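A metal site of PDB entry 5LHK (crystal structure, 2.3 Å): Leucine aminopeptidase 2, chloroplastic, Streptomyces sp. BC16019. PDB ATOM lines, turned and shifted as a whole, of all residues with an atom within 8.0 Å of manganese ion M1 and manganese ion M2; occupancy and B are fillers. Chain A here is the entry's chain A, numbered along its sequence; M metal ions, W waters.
The side-chain hydroxyl of Thr 373 is in hydrogen-bond range of the side-chain carboxylate of Asp 284 (2.9 Å).
OD1 of Asp 266 lies within hydrogen-bond range of N of Gly 268 (3.1 Å).
ND2 of Asn 316 is in hydrogen-bond range of OD1 of Asp 266, at 3.0 Å.
OD2 of Asp 343 lies within salt-bridge range of NZ of Lys 273 (2.8 Å).
The backbone carbonyl oxygen (O) of Thr 373 lies close to the side-chain amino group (NZ) of Lys 261 (3.0 Å).
O of Asp 284 sits at hydrogen-bond distance from N of Val 263 (3.4 Å).
The backbone NH (N) of Asp 266 lies within hydrogen-bond range of the backbone carbonyl oxygen (O) of Met 281, 3.1 Å away.
N of Asp 343 lies close to ND1 of His 341 (3.3 Å).
Four residues have an atom within 4 Å of manganese ion M1: Lys 261, Asp 266, Asp 284 and Glu 345.
Along chain A the residues within 4 Å of manganese ion M1 span positions 261 to 345.
Along chain A the residues within 4 Å of manganese ion M2 span positions 266 to 345.
The nearest printed residue that does not touch manganese ion M2 is Lys 273 (4.04 Å).
OD2 of Asp 284 binds manganese ion M1 (2.0 Å).
Manganese ion M1 is bound by OE2 of Glu 345 (2.1 Å).
Manganese ion M1 is bound by water W2, at 2.2 Å.
OD2 of Asp 266 is bound to manganese ion M1 (2.4 Å).
The side-chain amino group (NZ) of Lys 261 is bound to manganese ion M1 (2.4 Å).
OD2 of Asp 266 binds manganese ion M2.
The backbone carbonyl oxygen (O) of Asp 343 binds manganese ion M2.
OD1 of Asp 343 binds manganese ion M2.
The side-chain carboxylate (OE1) of Glu 345 binds manganese ion M2, 2.2 Å away.
Manganese ion M2 is bound by water W2 (2.3 Å).
Manganese ion M2 is bound by water W3 (2.6 Å).
Manganese ion M2 has six donor atoms within binding distance.
Water W1 bridges the side-chain carboxylate of Asp 284 and the backbone carbonyl oxygen of Thr 373.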
ATOM      1  N   VAL A 230      -5.541 -28.433  10.263  1.00  0.00           N
ATOM      2  CA  VAL A 230      -4.148 -28.090  10.527  1.00  0.00           C
ATOM      3  C   VAL A 230      -3.887 -27.785  12.009  1.00  0.00           C
ATOM      4  O   VAL A 230      -2.873 -28.228  12.565  1.00  0.00           O
ATOM      5  CB  VAL A 230      -3.691 -26.910   9.630  1.00  0.00           C
ATOM      6  CG1 VAL A 230      -2.368 -26.315  10.113  1.00  0.00           C
ATOM      7  CG2 VAL A 230      -3.569 -27.378   8.177  1.00  0.00           C
ATOM      8  N   LYS A 261      -1.785 -15.219   6.320  1.00  0.00           N
ATOM      9  CA  LYS A 261      -1.487 -16.507   6.934  1.00  0.00           C
ATOM     10  C   LYS A 261      -0.889 -16.308   8.335  1.00  0.00           C
ATOM     11  O   LYS A 261       0.180 -15.717   8.473  1.00  0.00           O
ATOM     12  CB  LYS A 261      -0.501 -17.287   6.075  1.00  0.00           C
ATOM     13  CG  LYS A 261      -0.062 -18.628   6.678  1.00  0.00           C
ATOM     14  CD  LYS A 261       1.116 -19.198   5.937  1.00  0.00           C
ATOM     15  CE  LYS A 261       1.668 -20.414   6.666  1.00  0.00           C
ATOM     16  NZ  LYS A 261       2.780 -21.008   5.878  1.00  0.00           N
ATOM     17  N   GLY A 262      -1.587 -16.806   9.349  1.00  0.00           N
ATOM     18  CA  GLY A 262      -1.191 -16.652  10.745  1.00  0.00           C
ATOM     19  C   GLY A 262      -0.852 -17.947  11.459  1.00  0.00           C
ATOM     20  O   GLY A 262      -1.380 -18.238  12.530  1.00  0.00           O
ATOM     21  N   VAL A 263       0.036 -18.736  10.895  1.00  0.00           N
ATOM     22  CA  VAL A 263       0.512 -19.934  11.591  1.00  0.00           C
ATOM     23  C   VAL A 263       1.530 -19.434  12.617  1.00  0.00           C
ATOM     24  O   VAL A 263       2.639 -19.040  12.268  1.00  0.00           O
ATOM     25  CB  VAL A 263       1.103 -20.987  10.627  1.00  0.00           C
ATOM     26  CG1 VAL A 263       1.669 -22.163  11.400  1.00  0.00           C
ATOM     27  CG2 VAL A 263       0.027 -21.460   9.654  1.00  0.00           C
ATOM     28  N   THR A 264       1.117 -19.424  13.874  1.00  0.00           N
ATOM     29  CA  THR A 264       1.911 -18.831  14.931  1.00  0.00           C
ATOM     30  C   THR A 264       3.136 -19.664  15.252  1.00  0.00           C
ATOM     31  O   THR A 264       4.114 -19.137  15.762  1.00  0.00           O
ATOM     32  CB  THR A 264       1.091 -18.591  16.201  1.00  0.00           C
ATOM     33  OG1 THR A 264       0.557 -19.830  16.674  1.00  0.00           O
ATOM     34  CG2 THR A 264      -0.028 -17.603  15.898  1.00  0.00           C
ATOM     35  N   PHE A 265       3.075 -20.964  14.961  1.00  0.00           N
ATOM     36  CA  PHE A 265       4.216 -21.852  15.088  1.00  0.00           C
ATOM     37  C   PHE A 265       4.062 -23.000  14.106  1.00  0.00           C
ATOM     38  O   PHE A 265       3.115 -23.780  14.207  1.00  0.00           O
ATOM     39  CB  PHE A 265       4.306 -22.399  16.507  1.00  0.00           C
ATOM     40  CG  PHE A 265       5.538 -23.226  16.756  1.00  0.00           C
ATOM     41  CD1 PHE A 265       6.794 -22.623  16.788  1.00  0.00           C
ATOM     42  CD2 PHE A 265       5.443 -24.602  16.910  1.00  0.00           C
ATOM     43  CE1 PHE A 265       7.940 -23.394  16.987  1.00  0.00           C
ATOM     44  CE2 PHE A 265       6.575 -25.375  17.108  1.00  0.00           C
ATOM     45  CZ  PHE A 265       7.830 -24.769  17.154  1.00  0.00           C
ATOM     46  N   ASP A 266       5.002 -23.092  13.175  1.00  0.00           N
ATOM     47  CA  ASP A 266       5.006 -24.169  12.188  1.00  0.00           C
ATOM     48  C   ASP A 266       6.123 -25.173  12.459  1.00  0.00           C
ATOM     49  O   ASP A 266       7.234 -25.000  11.979  1.00  0.00           O
ATOM     50  CB  ASP A 266       5.118 -23.576  10.775  1.00  0.00           C
ATOM     51  CG  ASP A 266       4.899 -24.608   9.684  1.00  0.00           C
ATOM     52  OD1 ASP A 266       4.515 -25.767   9.997  1.00  0.00           O
ATOM     53  OD2 ASP A 266       5.105 -24.260   8.494  1.00  0.00           O
ATOM     54  N   SER A 267       5.812 -26.231  13.202  1.00  0.00           N
ATOM     55  CA  SER A 267       6.756 -27.321  13.413  1.00  0.00           C
ATOM     56  C   SER A 267       6.895 -28.265  12.227  1.00  0.00           C
ATOM     57  O   SER A 267       7.829 -29.041  12.166  1.00  0.00           O
ATOM     58  CB  SER A 267       6.357 -28.170  14.613  1.00  0.00           C
ATOM     59  OG  SER A 267       5.297 -29.041  14.248  1.00  0.00           O
ATOM     60  N   GLY A 268       5.917 -28.225  11.332  1.00  0.00           N
ATOM     61  CA  GLY A 268       5.805 -29.185  10.253  1.00  0.00           C
ATOM     62  C   GLY A 268       4.656 -30.151  10.412  1.00  0.00           C
ATOM     63  O   GLY A 268       4.171 -30.689   9.428  1.00  0.00           O
ATOM     64  N   GLY A 269       4.212 -30.351  11.656  1.00  0.00           N
ATOM     65  CA  GLY A 269       3.223 -31.367  11.971  1.00  0.00           C
ATOM     66  C   GLY A 269       3.886 -32.742  12.025  1.00  0.00           C
ATOM     67  O   GLY A 269       5.041 -32.848  12.430  1.00  0.00           O
ATOM     68  N   SER A 271       4.789 -34.528   9.491  1.00  0.00           N
ATOM     69  CA  SER A 271       5.907 -34.317   8.585  1.00  0.00           C
ATOM     70  C   SER A 271       6.821 -33.278   9.228  1.00  0.00           C
ATOM     71  O   SER A 271       6.954 -32.112   8.777  1.00  0.00           O
ATOM     72  CB  SER A 271       5.422 -33.852   7.198  1.00  0.00           C
ATOM     73  OG  SER A 271       4.380 -34.692   6.676  1.00  0.00           O
ATOM     74  N   LYS A 273       9.603 -30.959  10.771  1.00  0.00           N
ATOM     75  CA  LYS A 273      10.769 -30.281  10.236  1.00  0.00           C
ATOM     76  C   LYS A 273      12.023 -30.913  10.840  1.00  0.00           C
ATOM     77  O   LYS A 273      12.056 -31.150  12.041  1.00  0.00           O
ATOM     78  CB  LYS A 273      10.740 -28.782  10.537  1.00  0.00           C
ATOM     79  CG  LYS A 273       9.765 -28.033   9.658  1.00  0.00           C
ATOM     80  CD  LYS A 273       9.653 -26.572  10.051  1.00  0.00           C
ATOM     81  CE  LYS A 273       8.521 -25.879   9.303  1.00  0.00           C
ATOM     82  NZ  LYS A 273       8.806 -25.781   7.859  1.00  0.00           N
ATOM     83  N   MET A 281      10.452 -20.941  13.030  1.00  0.00           N
ATOM     84  CA  MET A 281       9.130 -21.562  13.031  1.00  0.00           C
ATOM     85  C   MET A 281       8.057 -20.621  13.603  1.00  0.00           C
ATOM     86  O   MET A 281       6.910 -20.665  13.163  1.00  0.00           O
ATOM     87  CB  MET A 281       9.161 -22.905  13.815  1.00  0.00           C
ATOM     88  CG  MET A 281       9.922 -24.023  13.084  1.00  0.00           C
ATOM     89  SD  MET A 281      10.777 -25.283  14.050  1.00  0.00           S
ATOM     90  CE  MET A 281       9.563 -26.220  14.890  1.00  0.00           C
ATOM     91  N   ALA A 283       7.975 -17.485  13.009  1.00  0.00           N
ATOM     92  CA  ALA A 283       7.794 -16.417  12.023  1.00  0.00           C
ATOM     93  C   ALA A 283       6.804 -16.758  10.918  1.00  0.00           C
ATOM     94  O   ALA A 283       6.644 -15.977   9.975  1.00  0.00           O
ATOM     95  CB  ALA A 283       9.146 -16.054  11.387  1.00  0.00           C
ATOM     96  N   ASP A 284       6.100 -17.885  11.039  1.00  0.00           N
ATOM     97  CA  ASP A 284       5.222 -18.349   9.992  1.00  0.00           C
ATOM     98  C   ASP A 284       3.867 -17.609  10.015  1.00  0.00           C
ATOM     99  O   ASP A 284       2.937 -17.961   9.289  1.00  0.00           O
ATOM    100  CB  ASP A 284       5.057 -19.868  10.123  1.00  0.00           C
ATOM    101  CG  ASP A 284       4.697 -20.533   8.816  1.00  0.00           C
ATOM    102  OD1 ASP A 284       5.167 -20.071   7.749  1.00  0.00           O
ATOM    103  OD2 ASP A 284       3.956 -21.548   8.846  1.00  0.00           O
ATOM    104  N   MET A 285       3.759 -16.571  10.846  1.00  0.00           N
ATOM    105  CA  MET A 285       2.580 -15.697  10.913  1.00  0.00           C
ATOM    106  C   MET A 285       2.893 -14.292  10.370  1.00  0.00           C
ATOM    107  O   MET A 285       2.135 -13.354  10.615  1.00  0.00           O
ATOM    108  CB  MET A 285       2.012 -15.660  12.358  1.00  0.00           C
ATOM    109  CG  MET A 285       3.035 -15.576  13.502  1.00  0.00           C
ATOM    110  SD  MET A 285       4.265 -14.261  13.372  1.00  0.00           S
ATOM    111  CE  MET A 285       3.285 -12.821  13.698  1.00  0.00           C
ATOM    112  N   ASN A 316       0.867 -25.530  13.942  1.00  0.00           N
ATOM    113  CA  ASN A 316       1.040 -26.829  13.271  1.00  0.00           C
ATOM    114  C   ASN A 316       2.003 -27.693  14.084  1.00  0.00           C
ATOM    115  O   ASN A 316       3.212 -27.474  14.055  1.00  0.00           O
ATOM    116  CB  ASN A 316       1.541 -26.608  11.855  1.00  0.00           C
ATOM    117  CG  ASN A 316       1.582 -27.885  11.035  1.00  0.00           C
ATOM    118  OD1 ASN A 316       0.968 -28.899  11.383  1.00  0.00           O
ATOM    119  ND2 ASN A 316       2.326 -27.839   9.939  1.00  0.00           N
ATOM    120  N   HIS A 341       1.746 -33.897   2.417  1.00  0.00           N
ATOM    121  CA  HIS A 341       2.841 -33.429   3.255  1.00  0.00           C
ATOM    122  C   HIS A 341       2.264 -32.426   4.274  1.00  0.00           C
ATOM    123  O   HIS A 341       1.725 -31.378   3.868  1.00  0.00           O
ATOM    124  CB  HIS A 341       3.932 -32.782   2.392  1.00  0.00           C
ATOM    125  CG  HIS A 341       5.271 -32.712   3.050  1.00  0.00           C
ATOM    126  ND1 HIS A 341       5.497 -32.004   4.205  1.00  0.00           N
ATOM    127  CD2 HIS A 341       6.467 -33.251   2.710  1.00  0.00           C
ATOM    128  CE1 HIS A 341       6.764 -32.103   4.555  1.00  0.00           C
ATOM    129  NE2 HIS A 341       7.380 -32.863   3.667  1.00  0.00           N
ATOM    130  N   THR A 342       2.378 -32.718   5.581  1.00  0.00           N
ATOM    131  CA  THR A 342       1.736 -31.891   6.605  1.00  0.00           C
ATOM    132  C   THR A 342       2.391 -30.511   6.792  1.00  0.00           C
ATOM    133  O   THR A 342       1.815 -29.615   7.426  1.00  0.00           O
ATOM    134  CB  THR A 342       1.580 -32.588   7.976  1.00  0.00           C
ATOM    135  OG1 THR A 342       2.858 -32.783   8.606  1.00  0.00           O
ATOM    136  CG2 THR A 342       0.888 -33.921   7.834  1.00  0.00           C
ATOM    137  N   ASP A 343       3.614 -30.364   6.293  1.00  0.00           N
ATOM    138  CA  ASP A 343       4.342 -29.101   6.329  1.00  0.00           C
ATOM    139  C   ASP A 343       3.957 -28.102   5.226  1.00  0.00           C
ATOM    140  O   ASP A 343       4.421 -26.964   5.236  1.00  0.00           O
ATOM    141  CB  ASP A 343       5.856 -29.334   6.283  1.00  0.00           C
ATOM    142  CG  ASP A 343       6.655 -28.199   6.931  1.00  0.00           C
ATOM    143  OD1 ASP A 343       6.049 -27.287   7.559  1.00  0.00           O
ATOM    144  OD2 ASP A 343       7.892 -28.219   6.821  1.00  0.00           O
ATOM    145  N   ASN A 344       3.108 -28.512   4.287  1.00  0.00           N
ATOM    146  CA  ASN A 344       2.476 -27.565   3.363  1.00  0.00           C
ATOM    147  C   ASN A 344       1.076 -27.223   3.857  1.00  0.00           C
ATOM    148  O   ASN A 344       0.076 -27.362   3.147  1.00  0.00           O
ATOM    149  CB  ASN A 344       2.460 -28.110   1.924  1.00  0.00           C
ATOM    150  CG  ASN A 344       3.825 -28.038   1.260  1.00  0.00           C
ATOM    151  OD1 ASN A 344       4.824 -27.712   1.883  1.00  0.00           O
ATOM    152  ND2 ASN A 344       3.876 -28.354  -0.028  1.00  0.00           N
ATOM    153  N   GLU A 345       1.036 -26.733   5.090  1.00  0.00           N
ATOM    154  CA  GLU A 345      -0.203 -26.499   5.811  1.00  0.00           C
ATOM    155  C   GLU A 345      -0.818 -25.145   5.483  1.00  0.00           C
ATOM    156  O   GLU A 345      -2.043 -25.018   5.515  1.00  0.00           O
ATOM    157  CB  GLU A 345       0.020 -26.629   7.330  1.00  0.00           C
ATOM    158  CG  GLU A 345       0.529 -25.373   8.068  1.00  0.00           C
ATOM    159  CD  GLU A 345       1.908 -24.901   7.661  1.00  0.00           C
ATOM    160  OE1 GLU A 345       2.718 -25.733   7.213  1.00  0.00           O
ATOM    161  OE2 GLU A 345       2.189 -23.687   7.804  1.00  0.00           O
ATOM    162  N   GLY A 346       0.000 -24.148   5.182  1.00  0.00           N
ATOM    163  CA  GLY A 346      -0.505 -22.783   4.972  1.00  0.00           C
ATOM    164  C   GLY A 346      -1.534 -22.657   3.860  1.00  0.00           C
ATOM    165  O   GLY A 346      -2.540 -21.961   4.002  1.00  0.00           O
ATOM    166  N   ARG A 347      -1.274 -23.327   2.729  1.00  0.00           N
ATOM    167  CA  ARG A 347      -2.190 -23.250   1.588  1.00  0.00           C
ATOM    168  C   ARG A 347      -3.549 -23.868   1.924  1.00  0.00           C
ATOM    169  O   ARG A 347      -4.599 -23.375   1.477  1.00  0.00           O
ATOM    170  CB  ARG A 347      -1.559 -23.888   0.337  1.00  0.00           C
ATOM    171  CG  ARG A 347      -1.396 -25.411   0.381  1.00  0.00           C
ATOM    172  CD  ARG A 347      -0.397 -25.919  -0.652  1.00  0.00           C
ATOM    173  NE  ARG A 347       0.964 -25.505  -0.326  1.00  0.00           N
ATOM    174  CZ  ARG A 347       2.044 -25.657  -1.093  1.00  0.00           C
ATOM    175  NH1 ARG A 347       1.952 -26.240  -2.286  1.00  0.00           N
ATOM    176  NH2 ARG A 347       3.221 -25.214  -0.662  1.00  0.00           N
ATOM    177  N   ALA A 372       1.514 -14.264   2.729  1.00  0.00           N
ATOM    178  CA  ALA A 372       1.828 -15.523   3.376  1.00  0.00           C
ATOM    179  C   ALA A 372       3.318 -15.867   3.298  1.00  0.00           C
ATOM    180  O   ALA A 372       3.940 -15.772   2.238  1.00  0.00           O
ATOM    181  CB  ALA A 372       1.004 -16.627   2.741  1.00  0.00           C
ATOM    182  N   THR A 373       3.886 -16.276   4.430  1.00  0.00           N
ATOM    183  CA  THR A 373       5.194 -16.936   4.465  1.00  0.00           C
ATOM    184  C   THR A 373       4.980 -18.396   4.037  1.00  0.00           C
ATOM    185  O   THR A 373       4.993 -19.323   4.862  1.00  0.00           O
ATOM    186  CB  THR A 373       5.787 -16.868   5.877  1.00  0.00           C
ATOM    187  OG1 THR A 373       4.840 -17.366   6.821  1.00  0.00           O
ATOM    188  CG2 THR A 373       6.128 -15.412   6.240  1.00  0.00           C
ATOM    189  N   LEU A 374       4.743 -18.590   2.746  1.00  0.00           N
ATOM    190  CA  LEU A 374       4.095 -19.841   2.281  1.00  0.00           C
ATOM    191  C   LEU A 374       5.067 -20.940   1.874  1.00  0.00           C
ATOM    192  O   LEU A 374       4.898 -22.094   2.245  1.00  0.00           O
ATOM    193  CB  LEU A 374       3.134 -19.547   1.122  1.00  0.00           C
ATOM    194  CG  LEU A 374       2.092 -20.636   0.837  1.00  0.00           C
ATOM    195  CD1 LEU A 374       1.127 -20.834   2.011  1.00  0.00           C
ATOM    196  CD2 LEU A 374       1.315 -20.299  -0.433  1.00  0.00           C
ATOM    197  N   THR A 375       6.098 -20.574   1.160  1.00  0.00           N
ATOM    198  CA  THR A 375       6.882 -21.547   0.425  1.00  0.00           C
ATOM    199  C   THR A 375       8.374 -21.386   0.720  1.00  0.00           C
ATOM    200  O   THR A 375       8.881 -20.276   0.835  1.00  0.00           O
ATOM    201  CB  THR A 375       6.526 -21.381  -1.071  1.00  0.00           C
ATOM    202  OG1 THR A 375       5.257 -22.019  -1.323  1.00  0.00           O
ATOM    203  CG2 THR A 375       7.444 -22.004  -1.888  1.00  0.00           C
ATOM    204  N   SER A 376       9.067 -22.496   0.814  1.00  0.00           N
ATOM    205  CA  SER A 376      10.519 -22.486   0.982  1.00  0.00           C
ATOM    206  C   SER A 376      11.266 -22.669  -0.337  1.00  0.00           C
ATOM    207  O   SER A 376      12.459 -22.502  -0.365  1.00  0.00           O
ATOM    208  CB  SER A 376      10.925 -23.573   1.945  1.00  0.00           C
ATOM    209  OG  SER A 376      10.292 -24.775   1.574  1.00  0.00           O
ATOM    210  N   ALA A 464       8.019 -15.683   2.519  1.00  0.00           N
ATOM    211  CA  ALA A 464       8.672 -16.541   3.523  1.00  0.00           C
ATOM    212  C   ALA A 464      10.085 -16.073   3.844  1.00  0.00           C
ATOM    213  O   ALA A 464      10.410 -15.850   5.002  1.00  0.00           O
ATOM    214  CB  ALA A 464       8.697 -17.993   3.053  1.00  0.00           C
HETATM  215 MN    MN M   1       3.898 -22.693   7.186  1.00  0.00          MN
HETATM  216 MN    MN M   2       4.900 -25.599   6.834  1.00  0.00          MN
HETATM  217  O   HOH W   1       6.424 -21.881   5.894  1.00  0.00           O
HETATM  218  O   HOH W   2       4.719 -23.758   5.423  1.00  0.00           O
HETATM  219  O   HOH W   3       7.013 -25.060   5.493  1.00  0.00           O
